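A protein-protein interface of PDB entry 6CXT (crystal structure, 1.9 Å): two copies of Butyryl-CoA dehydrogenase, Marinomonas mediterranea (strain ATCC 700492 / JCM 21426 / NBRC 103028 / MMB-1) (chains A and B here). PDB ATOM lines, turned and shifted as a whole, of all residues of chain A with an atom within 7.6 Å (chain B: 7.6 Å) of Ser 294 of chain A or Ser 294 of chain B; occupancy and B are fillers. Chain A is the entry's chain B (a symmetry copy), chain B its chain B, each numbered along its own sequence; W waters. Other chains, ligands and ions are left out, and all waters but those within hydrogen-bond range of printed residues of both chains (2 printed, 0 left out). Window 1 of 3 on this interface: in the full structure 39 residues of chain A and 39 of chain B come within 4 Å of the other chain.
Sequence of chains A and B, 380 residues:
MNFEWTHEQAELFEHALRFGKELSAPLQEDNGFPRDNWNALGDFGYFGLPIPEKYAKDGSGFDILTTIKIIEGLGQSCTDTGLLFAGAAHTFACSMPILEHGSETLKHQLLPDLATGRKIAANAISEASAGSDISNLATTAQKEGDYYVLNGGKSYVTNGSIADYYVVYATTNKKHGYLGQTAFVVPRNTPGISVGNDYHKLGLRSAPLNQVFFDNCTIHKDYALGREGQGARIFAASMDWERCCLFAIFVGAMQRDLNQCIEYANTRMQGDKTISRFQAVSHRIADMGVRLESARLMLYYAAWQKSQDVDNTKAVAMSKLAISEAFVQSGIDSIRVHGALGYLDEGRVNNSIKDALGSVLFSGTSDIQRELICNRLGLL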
ATOM      1  N   VAL A 251     -13.622 -11.322  12.711  1.00  0.00           N
ATOM      2  CA  VAL A 251     -12.437 -11.698  11.937  1.00  0.00           C
ATOM      3  C   VAL A 251     -11.200 -11.054  12.603  1.00  0.00           C
ATOM      4  O   VAL A 251     -10.184 -11.727  12.834  1.00  0.00           O
ATOM      5  CB  VAL A 251     -12.542 -11.229  10.462  1.00  0.00           C
ATOM      6  CG1 VAL A 251     -11.201 -11.391   9.731  1.00  0.00           C
ATOM      7  CG2 VAL A 251     -13.648 -12.011   9.720  1.00  0.00           C
ATOM      8  N   MET A 288      -6.848 -23.149  13.130  1.00  0.00           N
ATOM      9  CA  MET A 288      -7.347 -21.789  13.425  1.00  0.00           C
ATOM     10  C   MET A 288      -6.893 -20.846  12.310  1.00  0.00           C
ATOM     11  O   MET A 288      -7.659 -19.978  11.852  1.00  0.00           O
ATOM     12  CB  MET A 288      -6.787 -21.291  14.778  1.00  0.00           C
ATOM     13  CG  MET A 288      -7.263 -22.072  15.988  1.00  0.00           C
ATOM     14  SD  MET A 288      -6.366 -21.583  17.509  1.00  0.00           S
ATOM     15  CE  MET A 288      -7.016 -19.923  17.700  1.00  0.00           C
ATOM     16  N   GLY A 289      -5.647 -21.000  11.850  1.00  0.00           N
ATOM     17  CA  GLY A 289      -5.146 -20.102  10.772  1.00  0.00           C
ATOM     18  C   GLY A 289      -5.916 -20.340   9.461  1.00  0.00           C
ATOM     19  O   GLY A 289      -6.280 -19.396   8.740  1.00  0.00           O
ATOM     20  N   VAL A 290      -6.170 -21.604   9.171  1.00  0.00           N
ATOM     21  CA  VAL A 290      -6.925 -21.960   7.953  1.00  0.00           C
ATOM     22  C   VAL A 290      -8.357 -21.348   7.993  1.00  0.00           C
ATOM     23  O   VAL A 290      -8.798 -20.662   7.039  1.00  0.00           O
ATOM     24  CB  VAL A 290      -7.000 -23.481   7.767  1.00  0.00           C
ATOM     25  CG1 VAL A 290      -7.924 -23.839   6.562  1.00  0.00           C
ATOM     26  CG2 VAL A 290      -5.570 -24.065   7.577  1.00  0.00           C
ATOM     27  N   ARG A 291      -9.053 -21.626   9.081  1.00  0.00           N
ATOM     28  CA  ARG A 291     -10.431 -21.150   9.198  1.00  0.00           C
ATOM     29  C   ARG A 291     -10.493 -19.608   9.187  1.00  0.00           C
ATOM     30  O   ARG A 291     -11.431 -19.045   8.628  1.00  0.00           O
ATOM     31  CB  ARG A 291     -11.079 -21.723  10.467  1.00  0.00           C
ATOM     32  CG  ARG A 291     -11.352 -23.242  10.325  1.00  0.00           C
ATOM     33  CD  ARG A 291     -12.189 -23.716  11.553  1.00  0.00           C
ATOM     34  NE  ARG A 291     -11.608 -23.219  12.843  1.00  0.00           N
ATOM     35  CZ  ARG A 291     -10.892 -23.951  13.717  1.00  0.00           C
ATOM     36  NH1 ARG A 291     -10.614 -25.220  13.457  1.00  0.00           N
ATOM     37  NH2 ARG A 291     -10.432 -23.369  14.844  1.00  0.00           N
ATOM     38  N   LEU A 292      -9.461 -18.951   9.734  1.00  0.00           N
ATOM     39  CA  LEU A 292      -9.413 -17.515   9.710  1.00  0.00           C
ATOM     40  C   LEU A 292      -9.146 -16.954   8.304  1.00  0.00           C
ATOM     41  O   LEU A 292      -9.821 -16.003   7.860  1.00  0.00           O
ATOM     42  CB  LEU A 292      -8.353 -17.018  10.705  1.00  0.00           C
ATOM     43  CG  LEU A 292      -8.119 -15.493  10.709  1.00  0.00           C
ATOM     44  CD1 LEU A 292      -9.452 -14.744  10.984  1.00  0.00           C
ATOM     45  CD2 LEU A 292      -7.130 -15.167  11.831  1.00  0.00           C
ATOM     46  N   GLU A 293      -8.169 -17.517   7.584  1.00  0.00           N
ATOM     47  CA  GLU A 293      -7.946 -17.046   6.192  1.00  0.00           C
ATOM     48  C   GLU A 293      -9.221 -17.189   5.372  1.00  0.00           C
ATOM     49  O   GLU A 293      -9.616 -16.271   4.643  1.00  0.00           O
ATOM     50  CB  GLU A 293      -6.771 -17.765   5.483  1.00  0.00           C
ATOM     51  CG  GLU A 293      -6.471 -17.099   4.132  1.00  0.00           C
ATOM     52  CD  GLU A 293      -5.615 -17.962   3.197  1.00  0.00           C
ATOM     53  OE1 GLU A 293      -6.196 -18.693   2.363  1.00  0.00           O
ATOM     54  OE2 GLU A 293      -4.362 -17.935   3.318  1.00  0.00           O
ATOM     55  N   SER A 294      -9.852 -18.350   5.509  1.00  0.00           N
ATOM     56  CA  SER A 294     -11.094 -18.627   4.854  1.00  0.00           C
ATOM     57  C   SER A 294     -12.182 -17.582   5.205  1.00  0.00           C
ATOM     58  O   SER A 294     -12.781 -16.998   4.284  1.00  0.00           O
ATOM     59  CB  SER A 294     -11.569 -20.000   5.305  1.00  0.00           C
ATOM     60  OG  SER A 294     -12.896 -20.247   4.820  1.00  0.00           O
ATOM     61  N   ALA A 295     -12.425 -17.359   6.503  1.00  0.00           N
ATOM     62  CA  ALA A 295     -13.522 -16.443   6.939  1.00  0.00           C
ATOM     63  C   ALA A 295     -13.249 -15.010   6.438  1.00  0.00           C
ATOM     64  O   ALA A 295     -14.185 -14.315   5.964  1.00  0.00           O
ATOM     65  CB  ALA A 295     -13.656 -16.475   8.454  1.00  0.00           C
ATOM     66  N   ARG A 296     -11.975 -14.583   6.507  1.00  0.00           N
ATOM     67  CA  ARG A 296     -11.557 -13.241   6.059  1.00  0.00           C
ATOM     68  C   ARG A 296     -11.794 -13.071   4.557  1.00  0.00           C
ATOM     69  O   ARG A 296     -12.291 -12.035   4.120  1.00  0.00           O
ATOM     70  CB  ARG A 296     -10.083 -12.975   6.415  1.00  0.00           C
ATOM     71  CG  ARG A 296      -9.611 -11.618   5.951  1.00  0.00           C
ATOM     72  CD  ARG A 296      -8.171 -11.341   6.311  1.00  0.00           C
ATOM     73  NE  ARG A 296      -7.971 -11.222   7.752  1.00  0.00           N
ATOM     74  CZ  ARG A 296      -7.165 -11.996   8.460  1.00  0.00           C
ATOM     75  NH1 ARG A 296      -6.480 -12.989   7.878  1.00  0.00           N
ATOM     76  NH2 ARG A 296      -6.993 -11.760   9.745  1.00  0.00           N
ATOM     77  N   LEU A 297     -11.380 -14.052   3.757  1.00  0.00           N
ATOM     78  CA  LEU A 297     -11.613 -13.990   2.311  1.00  0.00           C
ATOM     79  C   LEU A 297     -13.129 -13.949   1.996  1.00  0.00           C
ATOM     80  O   LEU A 297     -13.529 -13.299   1.047  1.00  0.00           O
ATOM     81  CB  LEU A 297     -11.002 -15.226   1.614  1.00  0.00           C
ATOM     82  CG  LEU A 297      -9.421 -15.155   1.598  1.00  0.00           C
ATOM     83  CD1 LEU A 297      -8.785 -16.473   1.126  1.00  0.00           C
ATOM     84  CD2 LEU A 297      -8.921 -14.001   0.708  1.00  0.00           C
ATOM     85  N   MET A 298     -13.928 -14.747   2.717  1.00  0.00           N
ATOM     86  CA  MET A 298     -15.364 -14.766   2.535  1.00  0.00           C
ATOM     87  C   MET A 298     -15.987 -13.423   2.849  1.00  0.00           C
ATOM     88  O   MET A 298     -16.898 -13.025   2.143  1.00  0.00           O
ATOM     89  CB  MET A 298     -16.014 -15.889   3.376  1.00  0.00           C
ATOM     90  CG  MET A 298     -15.522 -17.198   2.771  1.00  0.00           C
ATOM     91  SD  MET A 298     -16.153 -18.576   3.726  1.00  0.00           S
ATOM     92  CE  MET A 298     -17.854 -18.621   3.205  1.00  0.00           C
ATOM     93  N   LEU A 299     -15.459 -12.750   3.873  1.00  0.00           N
ATOM     94  CA  LEU A 299     -15.903 -11.392   4.235  1.00  0.00           C
ATOM     95  C   LEU A 299     -15.580 -10.415   3.098  1.00  0.00           C
ATOM     96  O   LEU A 299     -16.448  -9.641   2.671  1.00  0.00           O
ATOM     97  CB  LEU A 299     -15.161 -11.007   5.542  1.00  0.00           C
ATOM     98  CG  LEU A 299     -15.260  -9.536   5.993  1.00  0.00           C
ATOM     99  CD1 LEU A 299     -16.724  -9.182   6.341  1.00  0.00           C
ATOM    100  CD2 LEU A 299     -14.248  -9.199   7.109  1.00  0.00           C
ATOM    101  N   TYR A 300     -14.325 -10.446   2.644  1.00  0.00           N
ATOM    102  CA  TYR A 300     -13.855  -9.549   1.560  1.00  0.00           C
ATOM    103  C   TYR A 300     -14.691  -9.763   0.297  1.00  0.00           C
ATOM    104  O   TYR A 300     -15.155  -8.811  -0.322  1.00  0.00           O
ATOM    105  CB  TYR A 300     -12.365  -9.728   1.271  1.00  0.00           C
ATOM    106  CG  TYR A 300     -11.443  -9.293   2.395  1.00  0.00           C
ATOM    107  CD1 TYR A 300     -11.948  -8.598   3.545  1.00  0.00           C
ATOM    108  CD2 TYR A 300     -10.077  -9.617   2.349  1.00  0.00           C
ATOM    109  CE1 TYR A 300     -11.093  -8.214   4.555  1.00  0.00           C
ATOM    110  CE2 TYR A 300      -9.197  -9.221   3.367  1.00  0.00           C
ATOM    111  CZ  TYR A 300      -9.726  -8.544   4.476  1.00  0.00           C
ATOM    112  OH  TYR A 300      -8.884  -8.168   5.478  1.00  0.00           O
ATOM    113  N   MET A 318     -23.133 -16.712   3.655  1.00  0.00           N
ATOM    114  CA  MET A 318     -21.990 -17.619   3.826  1.00  0.00           C
ATOM    115  C   MET A 318     -20.926 -16.986   4.734  1.00  0.00           C
ATOM    116  O   MET A 318     -20.345 -17.678   5.582  1.00  0.00           O
ATOM    117  CB  MET A 318     -21.383 -17.986   2.462  1.00  0.00           C
ATOM    118  CG  MET A 318     -22.314 -18.887   1.649  1.00  0.00           C
ATOM    119  SD  MET A 318     -21.362 -19.438   0.203  1.00  0.00           S
ATOM    120  CE  MET A 318     -22.526 -20.693  -0.357  1.00  0.00           C
ATOM    121  N   SER A 319     -20.653 -15.704   4.566  1.00  0.00           N
ATOM    122  CA  SER A 319     -19.649 -15.025   5.348  1.00  0.00           C
ATOM    123  C   SER A 319     -20.028 -14.950   6.799  1.00  0.00           C
ATOM    124  O   SER A 319     -19.193 -15.252   7.705  1.00  0.00           O
ATOM    125  CB  SER A 319     -19.439 -13.635   4.775  1.00  0.00           C
ATOM    126  OG  SER A 319     -18.516 -12.889   5.526  1.00  0.00           O
ATOM    127  N   ALA A 322     -19.719 -18.478   8.223  1.00  0.00           N
ATOM    128  CA  ALA A 322     -18.337 -18.963   8.337  1.00  0.00           C
ATOM    129  C   ALA A 322     -17.620 -18.186   9.452  1.00  0.00           C
ATOM    130  O   ALA A 322     -16.869 -18.800  10.232  1.00  0.00           O
ATOM    131  CB  ALA A 322     -17.603 -18.798   7.018  1.00  0.00           C
ATOM    132  N   ILE A 323     -17.810 -16.853   9.514  1.00  0.00           N
ATOM    133  CA  ILE A 323     -17.115 -16.040  10.524  1.00  0.00           C
ATOM    134  C   ILE A 323     -17.569 -16.450  11.929  1.00  0.00           C
ATOM    135  O   ILE A 323     -16.725 -16.661  12.842  1.00  0.00           O
ATOM    136  CB  ILE A 323     -17.364 -14.510  10.306  1.00  0.00           C
ATOM    137  CG1 ILE A 323     -16.627 -14.060   9.033  1.00  0.00           C
ATOM    138  CG2 ILE A 323     -16.872 -13.683  11.527  1.00  0.00           C
ATOM    139  CD1 ILE A 323     -17.079 -12.686   8.533  1.00  0.00           C
ATOM    140  N   ALA A 326     -16.437 -19.988  12.790  1.00  0.00           N
ATOM    141  CA  ALA A 326     -14.980 -20.002  13.033  1.00  0.00           C
ATOM    142  C   ALA A 326     -14.659 -19.356  14.388  1.00  0.00           C
ATOM    143  O   ALA A 326     -13.767 -19.800  15.094  1.00  0.00           O
ATOM    144  CB  ALA A 326     -14.222 -19.327  11.885  1.00  0.00           C
ATOM    145  N   VAL B 251     -11.509 -27.894  -7.277  1.00  0.00           N
ATOM    146  CA  VAL B 251     -12.480 -26.819  -7.059  1.00  0.00           C
ATOM    147  C   VAL B 251     -13.543 -26.894  -8.179  1.00  0.00           C
ATOM    148  O   VAL B 251     -14.752 -26.852  -7.907  1.00  0.00           O
ATOM    149  CB  VAL B 251     -11.804 -25.423  -7.070  1.00  0.00           C
ATOM    150  CG1 VAL B 251     -12.850 -24.299  -7.106  1.00  0.00           C
ATOM    151  CG2 VAL B 251     -10.886 -25.254  -5.840  1.00  0.00           C
ATOM    152  N   MET B 288     -21.858 -27.737   1.602  1.00  0.00           N
ATOM    153  CA  MET B 288     -21.015 -27.971   0.410  1.00  0.00           C
ATOM    154  C   MET B 288     -20.769 -26.635  -0.290  1.00  0.00           C
ATOM    155  O   MET B 288     -19.650 -26.348  -0.754  1.00  0.00           O
ATOM    156  CB  MET B 288     -21.718 -28.942  -0.566  1.00  0.00           C
ATOM    157  CG  MET B 288     -21.913 -30.349  -0.033  1.00  0.00           C
ATOM    158  SD  MET B 288     -22.969 -31.356  -1.141  1.00  0.00           S
ATOM    159  CE  MET B 288     -21.854 -31.502  -2.538  1.00  0.00           C
ATOM    160  N   GLY B 289     -21.805 -25.794  -0.379  1.00  0.00           N
ATOM    161  CA  GLY B 289     -21.629 -24.481  -1.062  1.00  0.00           C
ATOM    162  C   GLY B 289     -20.657 -23.583  -0.276  1.00  0.00           C
ATOM    163  O   GLY B 289     -19.794 -22.899  -0.853  1.00  0.00           O
ATOM    164  N   VAL B 290     -20.796 -23.604   1.037  1.00  0.00           N
ATOM    165  CA  VAL B 290     -19.906 -22.805   1.902  1.00  0.00           C
ATOM    166  C   VAL B 290     -18.424 -23.253   1.731  1.00  0.00           C
ATOM    167  O   VAL B 290     -17.518 -22.422   1.477  1.00  0.00           O
ATOM    168  CB  VAL B 290     -20.324 -22.899   3.375  1.00  0.00           C
ATOM    169  CG1 VAL B 290     -19.289 -22.172   4.285  1.00  0.00           C
ATOM    170  CG2 VAL B 290     -21.754 -22.309   3.560  1.00  0.00           C
ATOM    171  N   ARG B 291     -18.209 -24.546   1.895  1.00  0.00           N
ATOM    172  CA  ARG B 291     -16.845 -25.068   1.814  1.00  0.00           C
ATOM    173  C   ARG B 291     -16.240 -24.838   0.414  1.00  0.00           C
ATOM    174  O   ARG B 291     -15.047 -24.565   0.307  1.00  0.00           O
ATOM    175  CB  ARG B 291     -16.829 -26.557   2.189  1.00  0.00           C
ATOM    176  CG  ARG B 291     -17.084 -26.761   3.704  1.00  0.00           C
ATOM    177  CD  ARG B 291     -16.853 -28.265   4.051  1.00  0.00           C
ATOM    178  NE  ARG B 291     -17.558 -29.170   3.086  1.00  0.00           N
ATOM    179  CZ  ARG B 291     -18.702 -29.837   3.326  1.00  0.00           C
ATOM    180  NH1 ARG B 291     -19.327 -29.698   4.487  1.00  0.00           N
ATOM    181  NH2 ARG B 291     -19.224 -30.621   2.361  1.00  0.00           N
ATOM    182  N   LEU B 292     -17.081 -24.873  -0.629  1.00  0.00           N
ATOM    183  CA  LEU B 292     -16.609 -24.608  -1.960  1.00  0.00           C
ATOM    184  C   LEU B 292     -16.251 -23.129  -2.179  1.00  0.00           C
ATOM    185  O   LEU B 292     -15.187 -22.810  -2.747  1.00  0.00           O
ATOM    186  CB  LEU B 292     -17.658 -25.072  -2.981  1.00  0.00           C
ATOM    187  CG  LEU B 292     -17.328 -24.753  -4.455  1.00  0.00           C
ATOM    188  CD1 LEU B 292     -15.952 -25.360  -4.842  1.00  0.00           C
ATOM    189  CD2 LEU B 292     -18.411 -25.386  -5.332  1.00  0.00           C
ATOM    190  N   GLU B 293     -17.118 -22.208  -1.744  1.00  0.00           N
ATOM    191  CA  GLU B 293     -16.757 -20.772  -1.872  1.00  0.00           C
ATOM    192  C   GLU B 293     -15.440 -20.490  -1.162  1.00  0.00           C
ATOM    193  O   GLU B 293     -14.557 -19.814  -1.703  1.00  0.00           O
ATOM    194  CB  GLU B 293     -17.859 -19.814  -1.352  1.00  0.00           C
ATOM    195  CG  GLU B 293     -17.509 -18.358  -1.692  1.00  0.00           C
ATOM    196  CD  GLU B 293     -18.314 -17.328  -0.890  1.00  0.00           C
ATOM    197  OE1 GLU B 293     -17.819 -16.881   0.169  1.00  0.00           O
ATOM    198  OE2 GLU B 293     -19.455 -16.992  -1.300  1.00  0.00           O
ATOM    199  N   SER B 294     -15.327 -21.023   0.050  1.00  0.00           N
ATOM    200  CA  SER B 294     -14.133 -20.902   0.830  1.00  0.00           C
ATOM    201  C   SER B 294     -12.891 -21.447   0.080  1.00  0.00           C
ATOM    202  O   SER B 294     -11.891 -20.719  -0.043  1.00  0.00           O
ATOM    203  CB  SER B 294     -14.324 -21.702   2.110  1.00  0.00           C
ATOM    204  OG  SER B 294     -13.091 -21.764   2.841  1.00  0.00           O
ATOM    205  N   ALA B 295     -12.962 -22.695  -0.401  1.00  0.00           N
ATOM    206  CA  ALA B 295     -11.784 -23.341  -1.052  1.00  0.00           C
ATOM    207  C   ALA B 295     -11.378 -22.558  -2.316  1.00  0.00           C
ATOM    208  O   ALA B 295     -10.163 -22.343  -2.567  1.00  0.00           O
ATOM    209  CB  ALA B 295     -12.103 -24.791  -1.386  1.00  0.00           C
ATOM    210  N   ARG B 296     -12.381 -22.103  -3.088  1.00  0.00           N
ATOM    211  CA  ARG B 296     -12.153 -21.332  -4.325  1.00  0.00           C
ATOM    212  C   ARG B 296     -11.457 -20.004  -4.015  1.00  0.00           C
ATOM    213  O   ARG B 296     -10.523 -19.614  -4.715  1.00  0.00           O
ATOM    214  CB  ARG B 296     -13.472 -21.095  -5.080  1.00  0.00           C
ATOM    215  CG  ARG B 296     -13.281 -20.287  -6.341  1.00  0.00           C
ATOM    216  CD  ARG B 296     -14.567 -20.066  -7.098  1.00  0.00           C
ATOM    217  NE  ARG B 296     -15.111 -21.304  -7.648  1.00  0.00           N
ATOM    218  CZ  ARG B 296     -16.304 -21.792  -7.350  1.00  0.00           C
ATOM    219  NH1 ARG B 296     -17.102 -21.168  -6.474  1.00  0.00           N
ATOM    220  NH2 ARG B 296     -16.736 -22.879  -7.958  1.00  0.00           N
ATOM    221  N   LEU B 297     -11.947 -19.274  -3.016  1.00  0.00           N
ATOM    222  CA  LEU B 297     -11.309 -18.013  -2.622  1.00  0.00           C
ATOM    223  C   LEU B 297      -9.855 -18.255  -2.149  1.00  0.00           C
ATOM    224  O   LEU B 297      -8.999 -17.419  -2.382  1.00  0.00           O
ATOM    225  CB  LEU B 297     -12.095 -17.348  -1.471  1.00  0.00           C
ATOM    226  CG  LEU B 297     -13.474 -16.762  -1.978  1.00  0.00           C
ATOM    227  CD1 LEU B 297     -14.376 -16.309  -0.818  1.00  0.00           C
ATOM    228  CD2 LEU B 297     -13.261 -15.583  -2.947  1.00  0.00           C
ATOM    229  N   MET B 298      -9.629 -19.328  -1.379  1.00  0.00           N
ATOM    230  CA  MET B 298      -8.303 -19.672  -0.907  1.00  0.00           C
ATOM    231  C   MET B 298      -7.361 -19.971  -2.053  1.00  0.00           C
ATOM    232  O   MET B 298      -6.208 -19.580  -1.976  1.00  0.00           O
ATOM    233  CB  MET B 298      -8.359 -20.854   0.087  1.00  0.00           C
ATOM    234  CG  MET B 298      -9.091 -20.327   1.316  1.00  0.00           C
ATOM    235  SD  MET B 298      -9.287 -21.647   2.510  1.00  0.00           S
ATOM    236  CE  MET B 298      -7.639 -21.776   3.171  1.00  0.00           C
ATOM    237  N   LEU B 299      -7.883 -20.622  -3.095  1.00  0.00           N
ATOM    238  CA  LEU B 299      -7.107 -20.900  -4.317  1.00  0.00           C
ATOM    239  C   LEU B 299      -6.728 -19.584  -5.007  1.00  0.00           C
ATOM    240  O   LEU B 299      -5.560 -19.376  -5.363  1.00  0.00           O
ATOM    241  CB  LEU B 299      -8.002 -21.782  -5.229  1.00  0.00           C
ATOM    242  CG  LEU B 299      -7.519 -22.001  -6.676  1.00  0.00           C
ATOM    243  CD1 LEU B 299      -6.187 -22.785  -6.682  1.00  0.00           C
ATOM    244  CD2 LEU B 299      -8.617 -22.618  -7.569  1.00  0.00           C
ATOM    245  N   TYR B 300      -7.729 -18.725  -5.212  1.00  0.00           N
ATOM    246  CA  TYR B 300      -7.524 -17.419  -5.884  1.00  0.00           C
ATOM    247  C   TYR B 300      -6.499 -16.584  -5.115  1.00  0.00           C
ATOM    248  O   TYR B 300      -5.573 -16.029  -5.697  1.00  0.00           O
ATOM    249  CB  TYR B 300      -8.835 -16.653  -6.062  1.00  0.00           C
ATOM    250  CG  TYR B 300      -9.820 -17.294  -7.022  1.00  0.00           C
ATOM    251  CD1 TYR B 300      -9.448 -18.423  -7.827  1.00  0.00           C
ATOM    252  CD2 TYR B 300     -11.139 -16.818  -7.098  1.00  0.00           C
ATOM    253  CE1 TYR B 300     -10.360 -18.991  -8.691  1.00  0.00           C
ATOM    254  CE2 TYR B 300     -12.071 -17.382  -7.981  1.00  0.00           C
ATOM    255  CZ  TYR B 300     -11.672 -18.486  -8.750  1.00  0.00           C
ATOM    256  OH  TYR B 300     -12.573 -19.052  -9.601  1.00  0.00           O
ATOM    257  N   MET B 318      -2.384 -23.763   2.783  1.00  0.00           N
ATOM    258  CA  MET B 318      -3.772 -23.658   3.250  1.00  0.00           C
ATOM    259  C   MET B 318      -4.753 -24.019   2.125  1.00  0.00           C
ATOM    260  O   MET B 318      -5.756 -24.703   2.374  1.00  0.00           O
ATOM    261  CB  MET B 318      -4.058 -22.243   3.780  1.00  0.00           C
ATOM    262  CG  MET B 318      -3.319 -21.965   5.089  1.00  0.00           C
ATOM    263  SD  MET B 318      -3.954 -20.381   5.712  1.00  0.00           S
ATOM    264  CE  MET B 318      -3.203 -20.475   7.346  1.00  0.00           C
ATOM    265  N   SER B 319      -4.494 -23.565   0.911  1.00  0.00           N
ATOM    266  CA  SER B 319      -5.370 -23.824  -0.206  1.00  0.00           C
ATOM    267  C   SER B 319      -5.415 -25.283  -0.554  1.00  0.00           C
ATOM    268  O   SER B 319      -6.522 -25.870  -0.752  1.00  0.00           O
ATOM    269  CB  SER B 319      -4.903 -23.003  -1.394  1.00  0.00           C
ATOM    270  OG  SER B 319      -5.673 -23.251  -2.543  1.00  0.00           O
ATOM    271  N   ALA B 322      -7.343 -27.041   2.233  1.00  0.00           N
ATOM    272  CA  ALA B 322      -8.779 -26.733   2.260  1.00  0.00           C
ATOM    273  C   ALA B 322      -9.458 -27.384   1.045  1.00  0.00           C
ATOM    274  O   ALA B 322     -10.565 -27.934   1.192  1.00  0.00           O
ATOM    275  CB  ALA B 322      -9.003 -25.230   2.251  1.00  0.00           C
ATOM    276  N   ILE B 323      -8.833 -27.299  -0.147  1.00  0.00           N
ATOM    277  CA  ILE B 323      -9.450 -27.856  -1.361  1.00  0.00           C
ATOM    278  C   ILE B 323      -9.587 -29.377  -1.228  1.00  0.00           C
ATOM    279  O   ILE B 323     -10.672 -29.952  -1.514  1.00  0.00           O
ATOM    280  CB  ILE B 323      -8.624 -27.504  -2.643  1.00  0.00           C
ATOM    281  CG1 ILE B 323      -8.762 -25.998  -2.927  1.00  0.00           C
ATOM    282  CG2 ILE B 323      -9.115 -28.325  -3.869  1.00  0.00           C
ATOM    283  CD1 ILE B 323      -7.731 -25.481  -3.934  1.00  0.00           C
ATOM    284  N   ALA B 326     -12.093 -30.325   1.486  1.00  0.00           N
ATOM    285  CA  ALA B 326     -13.465 -30.036   1.023  1.00  0.00           C
ATOM    286  C   ALA B 326     -13.906 -31.069  -0.024  1.00  0.00           C
ATOM    287  O   ALA B 326     -15.058 -31.474  -0.053  1.00  0.00           O
ATOM    288  CB  ALA B 326     -13.577 -28.601   0.491  1.00  0.00           C
HETATM  289  O   HOH W   1     -18.807 -14.749   1.202  1.00  0.00           O
HETATM  290  O   HOH W   2      -4.852 -19.660   0.403  1.00  0.00           O
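Gly 289 of chain A touches Met 318 of chain B, and with the chains exchanged Met 318 of chain A touches Gly 289 of chain B.
Glu 293 of chain A touches Met 318 of chain B, and with the chains exchanged Met 318 of chain A touches Glu 293 of chain B.
Ser 294 of chain A touches its own counterpart, Ser 294 of chain B.
Leu 297 of chain A touches Met 298 of chain B, and with the chains exchanged Met 298 of chain A touches Leu 297 of chain B.
Printed residues of chain B within 4 Å of Glu 293 of chain A: Met 298 (3.5 Å) and Met 318 (3.4 Å).
Printed residues of chain A within 4 Å of Gly 289 of chain B: Met 318.
Of the printed residues of chain A, Glu 293 of chain B touches Met 298 and Met 318.
Ser 294 of chain B touches two residues of chain A.
Of the printed residues of chain A, Met 298 of chain B touches Val 290, Glu 293, Ser 294 and Leu 297.
The nearest residue of chain B that does not touch Ser 294 of chain A is Leu 297 of chain B (5.4 Å).
The nearest residue of chain A that does not touch Ser 294 of chain B is Leu 297 of chain A (5.4 Å).
The side-chain sulfur of Met 318 of chain A lies close to the side-chain carboxylate of Glu 293 of chain B (3.4 Å).
The side-chain hydroxyl (OG) of Ser 294 of chain B is in hydrogen-bond range of the side-chain hydroxyl (OG) of Ser 294 of chain A, 2.5 Å away.
The side-chain carboxylate (OE2) of Glu 293 of chain A sits close to the side-chain sulfur (SD) of Met 318 of chain B, at 3.4 Å.
Among the printed residues, merely in contact across the chains: Gly 289 of chain A with Met 318 of chain B (3.4 Å), Met 318 of chain A with Gly 289 of chain B (3.4 Å), Met 298 of chain A with Glu 293 of chain B (3.5 Å), Glu 293 of chain A with Met 298 of chain B (3.5 Å), Leu 297 of chain A with Leu 297 of chain B (3.6 Å), Val 290 of chain A with Met 318 of chain B (3.7 Å), Met 318 of chain A with Val 290 of chain B (3.7 Å), Leu 297 of chain A with Met 298 of chain B (3.8 Å), Met 298 of chain A with Leu 297 of chain B (3.8 Å), Met 298 of chain A with Ser 294 of chain B (3.97 Å), Ser 294 of chain A with Met 298 of chain B (3.97 Å), Met 298 of chain A with Val 290 of chain B (3.98 Å) and Val 290 of chain A with Met 298 of chain B (3.98 Å).
Water W1 lies within hydrogen-bond range of the side-chain carboxylate (OE1) of Glu 293 of chain B and the backbone carbonyl oxygen (O) of Met 298 of chain A.
Water W2 bridges the side-chain carboxylate of Glu 293 of chain A and the backbone carbonyl oxygen of Met 298 of chain B.
Of the 19 printed residues of chain B, 7 touch a printed residue of chain A.
Printed residues of chain B that touch a printed residue of chain A: Gly 289, Val 290, Glu 293, Ser 294, Leu 297, Met 298 and Met 318.
Among the printed residues, no Asp or Glu carboxylate lies within 4 Å of a Lys or Arg side-chain nitrogen of the other chain.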
